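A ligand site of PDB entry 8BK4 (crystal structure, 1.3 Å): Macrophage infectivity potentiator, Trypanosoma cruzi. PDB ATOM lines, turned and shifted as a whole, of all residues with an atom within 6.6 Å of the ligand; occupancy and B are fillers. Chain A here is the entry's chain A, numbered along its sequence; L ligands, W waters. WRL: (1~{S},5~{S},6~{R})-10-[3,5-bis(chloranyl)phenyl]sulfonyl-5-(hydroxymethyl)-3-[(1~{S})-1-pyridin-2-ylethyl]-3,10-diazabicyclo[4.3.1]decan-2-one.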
ATOM      1  N   TYR A  61      -9.351 -30.696   0.331  1.00  0.00           N
ATOM      2  CA  TYR A  61     -10.375 -30.511  -0.686  1.00  0.00           C
ATOM      3  C   TYR A  61      -9.844 -30.682  -2.096  1.00  0.00           C
ATOM      4  O   TYR A  61      -8.650 -30.599  -2.364  1.00  0.00           O
ATOM      5  CB  TYR A  61     -11.046 -29.133  -0.596  1.00  0.00           C
ATOM      6  CG  TYR A  61     -10.182 -27.977  -1.070  1.00  0.00           C
ATOM      7  CD1 TYR A  61      -9.253 -27.411  -0.223  1.00  0.00           C
ATOM      8  CD2 TYR A  61     -10.290 -27.444  -2.370  1.00  0.00           C
ATOM      9  CE1 TYR A  61      -8.463 -26.349  -0.636  1.00  0.00           C
ATOM     10  CE2 TYR A  61      -9.500 -26.383  -2.783  1.00  0.00           C
ATOM     11  CZ  TYR A  61      -8.581 -25.837  -1.902  1.00  0.00           C
ATOM     12  OH  TYR A  61      -7.754 -24.795  -2.245  1.00  0.00           O
ATOM     13  N   GLY A  63     -11.494 -29.247  -5.932  1.00  0.00           N
ATOM     14  CA  GLY A  63     -12.528 -28.473  -6.589  1.00  0.00           C
ATOM     15  C   GLY A  63     -12.607 -28.836  -8.054  1.00  0.00           C
ATOM     16  O   GLY A  63     -11.575 -28.960  -8.715  1.00  0.00           O
ATOM     17  N   PHE A  71      -9.770 -28.064 -10.821  1.00  0.00           N
ATOM     18  CA  PHE A  71      -9.136 -26.772 -10.965  1.00  0.00           C
ATOM     19  C   PHE A  71      -8.342 -26.318  -9.744  1.00  0.00           C
ATOM     20  O   PHE A  71      -7.533 -25.396  -9.878  1.00  0.00           O
ATOM     21  CB  PHE A  71     -10.162 -25.682 -11.319  1.00  0.00           C
ATOM     22  CG  PHE A  71     -11.150 -25.375 -10.224  1.00  0.00           C
ATOM     23  CD1 PHE A  71     -10.843 -24.421  -9.266  1.00  0.00           C
ATOM     24  CD2 PHE A  71     -12.371 -26.001 -10.156  1.00  0.00           C
ATOM     25  CE1 PHE A  71     -11.727 -24.135  -8.257  1.00  0.00           C
ATOM     26  CE2 PHE A  71     -13.255 -25.715  -9.147  1.00  0.00           C
ATOM     27  CZ  PHE A  71     -12.932 -24.782  -8.197  1.00  0.00           C
ATOM     28  N   ASP A  72      -8.495 -26.977  -8.594  1.00  0.00           N
ATOM     29  CA  ASP A  72      -7.732 -26.658  -7.409  1.00  0.00           C
ATOM     30  C   ASP A  72      -7.868 -27.825  -6.441  1.00  0.00           C
ATOM     31  O   ASP A  72      -8.855 -28.580  -6.479  1.00  0.00           O
ATOM     32  CB  ASP A  72      -8.233 -25.366  -6.759  1.00  0.00           C
ATOM     33  CG  ASP A  72      -7.290 -24.845  -5.674  1.00  0.00           C
ATOM     34  OD1 ASP A  72      -6.073 -25.162  -5.706  1.00  0.00           O
ATOM     35  OD2 ASP A  72      -7.800 -24.111  -4.792  1.00  0.00           O
ATOM     36  N   SER A  73      -6.895 -27.936  -5.547  1.00  0.00           N
ATOM     37  CA  SER A  73      -6.904 -29.001  -4.563  1.00  0.00           C
ATOM     38  C   SER A  73      -5.833 -28.730  -3.514  1.00  0.00           C
ATOM     39  O   SER A  73      -4.813 -28.084  -3.792  1.00  0.00           O
ATOM     40  CB  SER A  73      -6.637 -30.352  -5.184  1.00  0.00           C
ATOM     41  OG  SER A  73      -5.296 -30.378  -5.673  1.00  0.00           O
ATOM     42  N   ARG A  77      -1.515 -27.590  -3.481  1.00  0.00           N
ATOM     43  CA  ARG A  77      -1.030 -26.492  -2.662  1.00  0.00           C
ATOM     44  C   ARG A  77       0.141 -26.894  -1.779  1.00  0.00           C
ATOM     45  O   ARG A  77       0.935 -26.040  -1.387  1.00  0.00           O
ATOM     46  CB  ARG A  77      -2.149 -25.985  -1.741  1.00  0.00           C
ATOM     47  CG  ARG A  77      -3.433 -25.585  -2.472  1.00  0.00           C
ATOM     48  CD  ARG A  77      -3.331 -24.159  -2.902  1.00  0.00           C
ATOM     49  NE  ARG A  77      -4.535 -23.664  -3.545  1.00  0.00           N
ATOM     50  CZ  ARG A  77      -4.739 -22.377  -3.775  1.00  0.00           C
ATOM     51  NH1 ARG A  77      -3.910 -21.461  -3.314  1.00  0.00           N
ATOM     52  NH2 ARG A  77      -5.790 -22.001  -4.513  1.00  0.00           N
ATOM     53  N   PHE A  83      -8.986 -22.492   6.562  1.00  0.00           N
ATOM     54  CA  PHE A  83      -9.957 -21.444   6.278  1.00  0.00           C
ATOM     55  C   PHE A  83     -10.885 -21.254   7.477  1.00  0.00           C
ATOM     56  O   PHE A  83     -11.188 -22.191   8.201  1.00  0.00           O
ATOM     57  CB  PHE A  83     -10.852 -21.803   5.074  1.00  0.00           C
ATOM     58  CG  PHE A  83     -10.098 -22.209   3.832  1.00  0.00           C
ATOM     59  CD1 PHE A  83      -9.651 -21.253   2.947  1.00  0.00           C
ATOM     60  CD2 PHE A  83      -9.830 -23.538   3.559  1.00  0.00           C
ATOM     61  CE1 PHE A  83      -8.945 -21.626   1.792  1.00  0.00           C
ATOM     62  CE2 PHE A  83      -9.124 -23.911   2.404  1.00  0.00           C
ATOM     63  CZ  PHE A  83      -8.692 -22.955   1.535  1.00  0.00           C
ATOM     64  N   GLU A  87     -14.307 -16.569   5.550  1.00  0.00           N
ATOM     65  CA  GLU A  87     -13.325 -16.170   4.547  1.00  0.00           C
ATOM     66  C   GLU A  87     -13.655 -16.713   3.159  1.00  0.00           C
ATOM     67  O   GLU A  87     -13.048 -16.282   2.186  1.00  0.00           O
ATOM     68  CB  GLU A  87     -11.948 -16.717   4.935  1.00  0.00           C
ATOM     69  CG  GLU A  87     -11.269 -15.946   6.041  1.00  0.00           C
ATOM     70  CD  GLU A  87     -10.094 -16.700   6.689  1.00  0.00           C
ATOM     71  OE1 GLU A  87      -9.766 -17.849   6.293  1.00  0.00           O
ATOM     72  OE2 GLU A  87      -9.496 -16.110   7.623  1.00  0.00           O
ATOM     73  N   VAL A  88     -14.568 -17.668   3.071  1.00  0.00           N
ATOM     74  CA  VAL A  88     -14.739 -18.467   1.862  1.00  0.00           C
ATOM     75  C   VAL A  88     -16.099 -18.193   1.222  1.00  0.00           C
ATOM     76  O   VAL A  88     -16.958 -17.512   1.791  1.00  0.00           O
ATOM     77  CB  VAL A  88     -14.541 -19.979   2.145  1.00  0.00           C
ATOM     78  CG1 VAL A  88     -13.061 -20.299   2.367  1.00  0.00           C
ATOM     79  CG2 VAL A  88     -15.372 -20.419   3.322  1.00  0.00           C
ATOM     80  N   ILE A  89     -16.289 -18.747   0.026  1.00  0.00           N
ATOM     81  CA  ILE A  89     -17.560 -18.582  -0.682  1.00  0.00           C
ATOM     82  C   ILE A  89     -18.722 -19.127   0.158  1.00  0.00           C
ATOM     83  O   ILE A  89     -18.562 -20.027   0.998  1.00  0.00           O
ATOM     84  CB  ILE A  89     -17.517 -19.219  -2.085  1.00  0.00           C
ATOM     85  CG1 ILE A  89     -17.061 -20.706  -2.029  1.00  0.00           C
ATOM     86  CG2 ILE A  89     -16.588 -18.433  -3.014  1.00  0.00           C
ATOM     87  CD1 ILE A  89     -17.238 -21.457  -3.349  1.00  0.00           C
ATOM     88  N   LYS A  90     -19.918 -18.555  -0.081  1.00  0.00           N
ATOM     89  CA  LYS A  90     -21.067 -18.841   0.794  1.00  0.00           C
ATOM     90  C   LYS A  90     -21.415 -20.323   0.871  1.00  0.00           C
ATOM     91  O   LYS A  90     -21.845 -20.804   1.921  1.00  0.00           O
ATOM     92  CB  LYS A  90     -22.336 -18.039   0.437  1.00  0.00           C
ATOM     93  CG  LYS A  90     -22.199 -16.533   0.477  1.00  0.00           C
ATOM     94  CD  LYS A  90     -23.283 -15.863  -0.355  1.00  0.00           C
ATOM     95  CE  LYS A  90     -22.691 -14.919  -1.416  1.00  0.00           C
ATOM     96  NZ  LYS A  90     -22.494 -15.614  -2.713  1.00  0.00           N
ATOM     97  N   TRP A  92     -19.349 -22.820   0.872  1.00  0.00           N
ATOM     98  CA  TRP A  92     -18.443 -23.372   1.872  1.00  0.00           C
ATOM     99  C   TRP A  92     -18.751 -22.848   3.267  1.00  0.00           C
ATOM    100  O   TRP A  92     -18.658 -23.594   4.247  1.00  0.00           O
ATOM    101  CB  TRP A  92     -17.001 -22.989   1.562  1.00  0.00           C
ATOM    102  CG  TRP A  92     -16.256 -23.897   0.644  1.00  0.00           C
ATOM    103  CD1 TRP A  92     -16.600 -24.304  -0.605  1.00  0.00           C
ATOM    104  CD2 TRP A  92     -14.995 -24.513   0.951  1.00  0.00           C
ATOM    105  NE1 TRP A  92     -15.607 -25.118  -1.122  1.00  0.00           N
ATOM    106  CE2 TRP A  92     -14.619 -25.284  -0.175  1.00  0.00           C
ATOM    107  CE3 TRP A  92     -14.137 -24.486   2.056  1.00  0.00           C
ATOM    108  CZ2 TRP A  92     -13.415 -25.994  -0.224  1.00  0.00           C
ATOM    109  CZ3 TRP A  92     -12.965 -25.222   2.016  1.00  0.00           C
ATOM    110  CH2 TRP A  92     -12.621 -25.969   0.884  1.00  0.00           C
ATOM    111  N   TYR A 115     -18.950 -17.845  -7.037  1.00  0.00           N
ATOM    112  CA  TYR A 115     -18.390 -16.602  -7.567  1.00  0.00           C
ATOM    113  C   TYR A 115     -19.372 -15.804  -8.424  1.00  0.00           C
ATOM    114  O   TYR A 115     -19.002 -14.782  -9.035  1.00  0.00           O
ATOM    115  CB  TYR A 115     -17.070 -16.876  -8.302  1.00  0.00           C
ATOM    116  CG  TYR A 115     -16.005 -17.297  -7.327  1.00  0.00           C
ATOM    117  CD1 TYR A 115     -15.262 -16.362  -6.625  1.00  0.00           C
ATOM    118  CD2 TYR A 115     -15.806 -18.629  -7.013  1.00  0.00           C
ATOM    119  CE1 TYR A 115     -14.306 -16.745  -5.690  1.00  0.00           C
ATOM    120  CE2 TYR A 115     -14.881 -19.029  -6.068  1.00  0.00           C
ATOM    121  CZ  TYR A 115     -14.130 -18.093  -5.402  1.00  0.00           C
ATOM    122  OH  TYR A 115     -13.240 -18.487  -4.465  1.00  0.00           O
ATOM    123  N   GLY A 119     -17.297 -14.640 -11.510  1.00  0.00           N
ATOM    124  CA  GLY A 119     -16.290 -15.667 -11.712  1.00  0.00           C
ATOM    125  C   GLY A 119     -15.074 -15.386 -10.846  1.00  0.00           C
ATOM    126  O   GLY A 119     -15.078 -14.502  -9.992  1.00  0.00           O
ATOM    127  N   GLY A 120     -14.025 -16.144 -11.078  1.00  0.00           N
ATOM    128  CA  GLY A 120     -12.858 -15.957 -10.225  1.00  0.00           C
ATOM    129  C   GLY A 120     -11.560 -16.586 -10.689  1.00  0.00           C
ATOM    130  O   GLY A 120     -11.548 -17.601 -11.400  1.00  0.00           O
ATOM    131  N   GLY A 121     -10.449 -15.961 -10.273  1.00  0.00           N
ATOM    132  CA  GLY A 121      -9.099 -16.515 -10.414  1.00  0.00           C
ATOM    133  C   GLY A 121      -8.661 -16.845 -11.817  1.00  0.00           C
ATOM    134  O   GLY A 121      -7.639 -17.520 -12.007  1.00  0.00           O
ATOM    135  N   GLY A 122      -9.403 -16.378 -12.814  1.00  0.00           N
ATOM    136  CA  GLY A 122      -9.071 -16.653 -14.202  1.00  0.00           C
ATOM    137  C   GLY A 122      -9.437 -18.030 -14.689  1.00  0.00           C
ATOM    138  O   GLY A 122      -9.233 -18.318 -15.878  1.00  0.00           O
ATOM    139  N   MET A 123      -9.963 -18.922 -13.831  1.00  0.00           N
ATOM    140  CA  MET A 123     -10.353 -20.236 -14.291  1.00  0.00           C
ATOM    141  C   MET A 123     -11.793 -20.589 -13.989  1.00  0.00           C
ATOM    142  O   MET A 123     -12.269 -21.616 -14.481  1.00  0.00           O
ATOM    143  CB  MET A 123      -9.449 -21.351 -13.719  1.00  0.00           C
ATOM    144  CG  MET A 123      -9.605 -21.764 -12.250  1.00  0.00           C
ATOM    145  SD  MET A 123      -9.181 -20.526 -11.057  1.00  0.00           S
ATOM    146  CE  MET A 123      -7.408 -20.744 -11.056  1.00  0.00           C
ATOM    147  N   ILE A 124     -12.506 -19.780 -13.203  1.00  0.00           N
ATOM    148  CA  ILE A 124     -13.913 -20.027 -12.903  1.00  0.00           C
ATOM    149  C   ILE A 124     -14.725 -18.994 -13.681  1.00  0.00           C
ATOM    150  O   ILE A 124     -14.665 -17.807 -13.355  1.00  0.00           O
ATOM    151  CB  ILE A 124     -14.189 -19.948 -11.397  1.00  0.00           C
ATOM    152  CG1 ILE A 124     -13.358 -20.991 -10.649  1.00  0.00           C
ATOM    153  CG2 ILE A 124     -15.663 -20.143 -11.118  1.00  0.00           C
ATOM    154  CD1 ILE A 124     -13.304 -20.800  -9.139  1.00  0.00           C
ATOM    155  N   LEU A 130     -20.058 -25.032  -8.857  1.00  0.00           N
ATOM    156  CA  LEU A 130     -18.802 -25.660  -8.506  1.00  0.00           C
ATOM    157  C   LEU A 130     -19.076 -26.957  -7.759  1.00  0.00           C
ATOM    158  O   LEU A 130     -20.047 -27.069  -7.008  1.00  0.00           O
ATOM    159  CB  LEU A 130     -17.926 -24.752  -7.655  1.00  0.00           C
ATOM    160  CG  LEU A 130     -17.503 -23.452  -8.298  1.00  0.00           C
ATOM    161  CD1 LEU A 130     -16.778 -22.612  -7.288  1.00  0.00           C
ATOM    162  CD2 LEU A 130     -16.658 -23.669  -9.533  1.00  0.00           C
ATOM    163  N   PHE A 132     -17.192 -29.686  -5.106  1.00  0.00           N
ATOM    164  CA  PHE A 132     -16.061 -29.861  -4.204  1.00  0.00           C
ATOM    165  C   PHE A 132     -16.179 -31.199  -3.489  1.00  0.00           C
ATOM    166  O   PHE A 132     -17.268 -31.648  -3.118  1.00  0.00           O
ATOM    167  CB  PHE A 132     -15.940 -28.762  -3.158  1.00  0.00           C
ATOM    168  CG  PHE A 132     -15.480 -27.433  -3.694  1.00  0.00           C
ATOM    169  CD1 PHE A 132     -16.412 -26.484  -4.122  1.00  0.00           C
ATOM    170  CD2 PHE A 132     -14.135 -27.111  -3.736  1.00  0.00           C
ATOM    171  CE1 PHE A 132     -15.992 -25.243  -4.620  1.00  0.00           C
ATOM    172  CE2 PHE A 132     -13.694 -25.874  -4.209  1.00  0.00           C
ATOM    173  CZ  PHE A 132     -14.620 -24.946  -4.643  1.00  0.00           C
HETATM  174  N1  WRL L   1     -11.774 -21.695  -3.223  1.00  0.00           N
HETATM  175  N3  WRL L   1      -9.992 -15.844  -1.716  1.00  0.00           N
HETATM  176  C4  WRL L   1     -12.869 -21.091  -2.463  1.00  0.00           C
HETATM  177  C5  WRL L   1     -13.234 -22.159  -1.417  1.00  0.00           C
HETATM  178  C6  WRL L   1     -12.024 -22.564  -0.572  1.00  0.00           C
HETATM  179  C7  WRL L   1     -10.903 -23.073  -1.461  1.00  0.00           C
HETATM  180  C8  WRL L   1     -10.525 -22.038  -2.515  1.00  0.00           C
HETATM  181  C10 WRL L   1      -8.275 -21.006  -2.224  1.00  0.00           C
HETATM  182  C13 WRL L   1     -10.681 -17.757   0.104  1.00  0.00           C
HETATM  183  C15 WRL L   1      -9.538 -14.922  -2.575  1.00  0.00           C
HETATM  184  C17 WRL L   1     -11.001 -15.605  -4.285  1.00  0.00           C
HETATM  185  C20 WRL L   1      -9.624 -21.855  -6.173  1.00  0.00           C
HETATM  186  C21 WRL L   1      -8.783 -21.103  -6.986  1.00  0.00           C
HETATM  187  C22 WRL L   1      -9.104 -19.838  -7.421  1.00  0.00           C
HETATM  188  C1  WRL L   1     -10.313 -19.310  -7.002  1.00  0.00           C
HETATM  189  C11 WRL L   1     -10.288 -19.501  -2.517  1.00  0.00           C
HETATM  190  C12 WRL L   1     -11.478 -17.731  -1.191  1.00  0.00           C
HETATM  191  C14 WRL L   1     -10.963 -16.670  -2.155  1.00  0.00           C
HETATM  192  C16 WRL L   1     -10.008 -14.762  -3.853  1.00  0.00           C
HETATM  193  C18 WRL L   1     -11.479 -16.565  -3.421  1.00  0.00           C
HETATM  194  C19 WRL L   1     -12.693 -19.759  -1.757  1.00  0.00           C
HETATM  195  C2  WRL L   1     -11.176 -20.028  -6.200  1.00  0.00           C
HETATM  196  C3  WRL L   1     -10.822 -21.288  -5.766  1.00  0.00           C
HETATM  197  C9  WRL L   1      -9.761 -20.834  -1.954  1.00  0.00           C
HETATM  198  N2  WRL L   1     -11.527 -19.064  -1.849  1.00  0.00           N
HETATM  199  O1  WRL L   1     -11.445 -23.560  -4.777  1.00  0.00           O
HETATM  200  O2  WRL L   1      -7.556 -20.083  -1.418  1.00  0.00           O
HETATM  201  O3  WRL L   1     -13.653 -19.321  -1.121  1.00  0.00           O
HETATM  202  O4  WRL L   1     -13.268 -21.927  -5.151  1.00  0.00           O
HETATM  203  S1  WRL L   1     -11.926 -22.216  -4.742  1.00  0.00           S
HETATM  204 CL1  WRL L   1     -10.759 -17.718  -7.525  1.00  0.00          CL
HETATM  205 CL2  WRL L   1      -7.284 -21.810  -7.493  1.00  0.00          CL
HETATM  206  O   HOH W   1      -5.578 -21.115   0.322  1.00  0.00           O
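The side-chain carboxylate of Asp 72 lies within salt-bridge range of the guanidinium group of Arg 77, 2.9 Å away.
OH of Tyr 61 is in hydrogen-bond range of OD2 of Asp 72, 2.6 Å away.
The backbone carbonyl oxygen of Asp 72 is in hydrogen-bond range of the backbone NH of Gly 63, at 2.8 Å.
The backbone carbonyl oxygen (O) of Gly 63 lies within hydrogen-bond range of the backbone NH (N) of Phe 71, at 2.9 Å.
Tyr 61 touches the ligand (CZ to C7, 3.6 Å).
Phe 71 touches the ligand.
Asp 72 touches the ligand (OD2 to C20, 3.2 Å).
NH2 of Arg 77 touches CL2 of the ligand (3.3 Å).
CZ of Phe 83 touches C7 of the ligand, 3.7 Å away.
O of Glu 87 touches C13 of the ligand (3.5 Å).
Val 88 touches the ligand.
Trp 92 touches the ligand (CE2 to C5, 3.6 Å).
Gly 120 touches the ligand.
Gly 121 touches the ligand (N to CL1, 3.3 Å).
Met 123 touches the ligand.
CD1 of Ile 124 touches C2 of the ligand, 3.7 Å away.
Phe 132 touches the ligand.
The nearest printed residue that does not touch the ligand is Leu 130 (4.2 Å).
The side-chain hydroxyl (OH) of Tyr 115 sits close to an oxygen (O3) of the ligand (3.5 Å).
An oxygen (O3) of the ligand is in hydrogen-bond range of the backbone NH of Ile 89 (2.9 Å).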
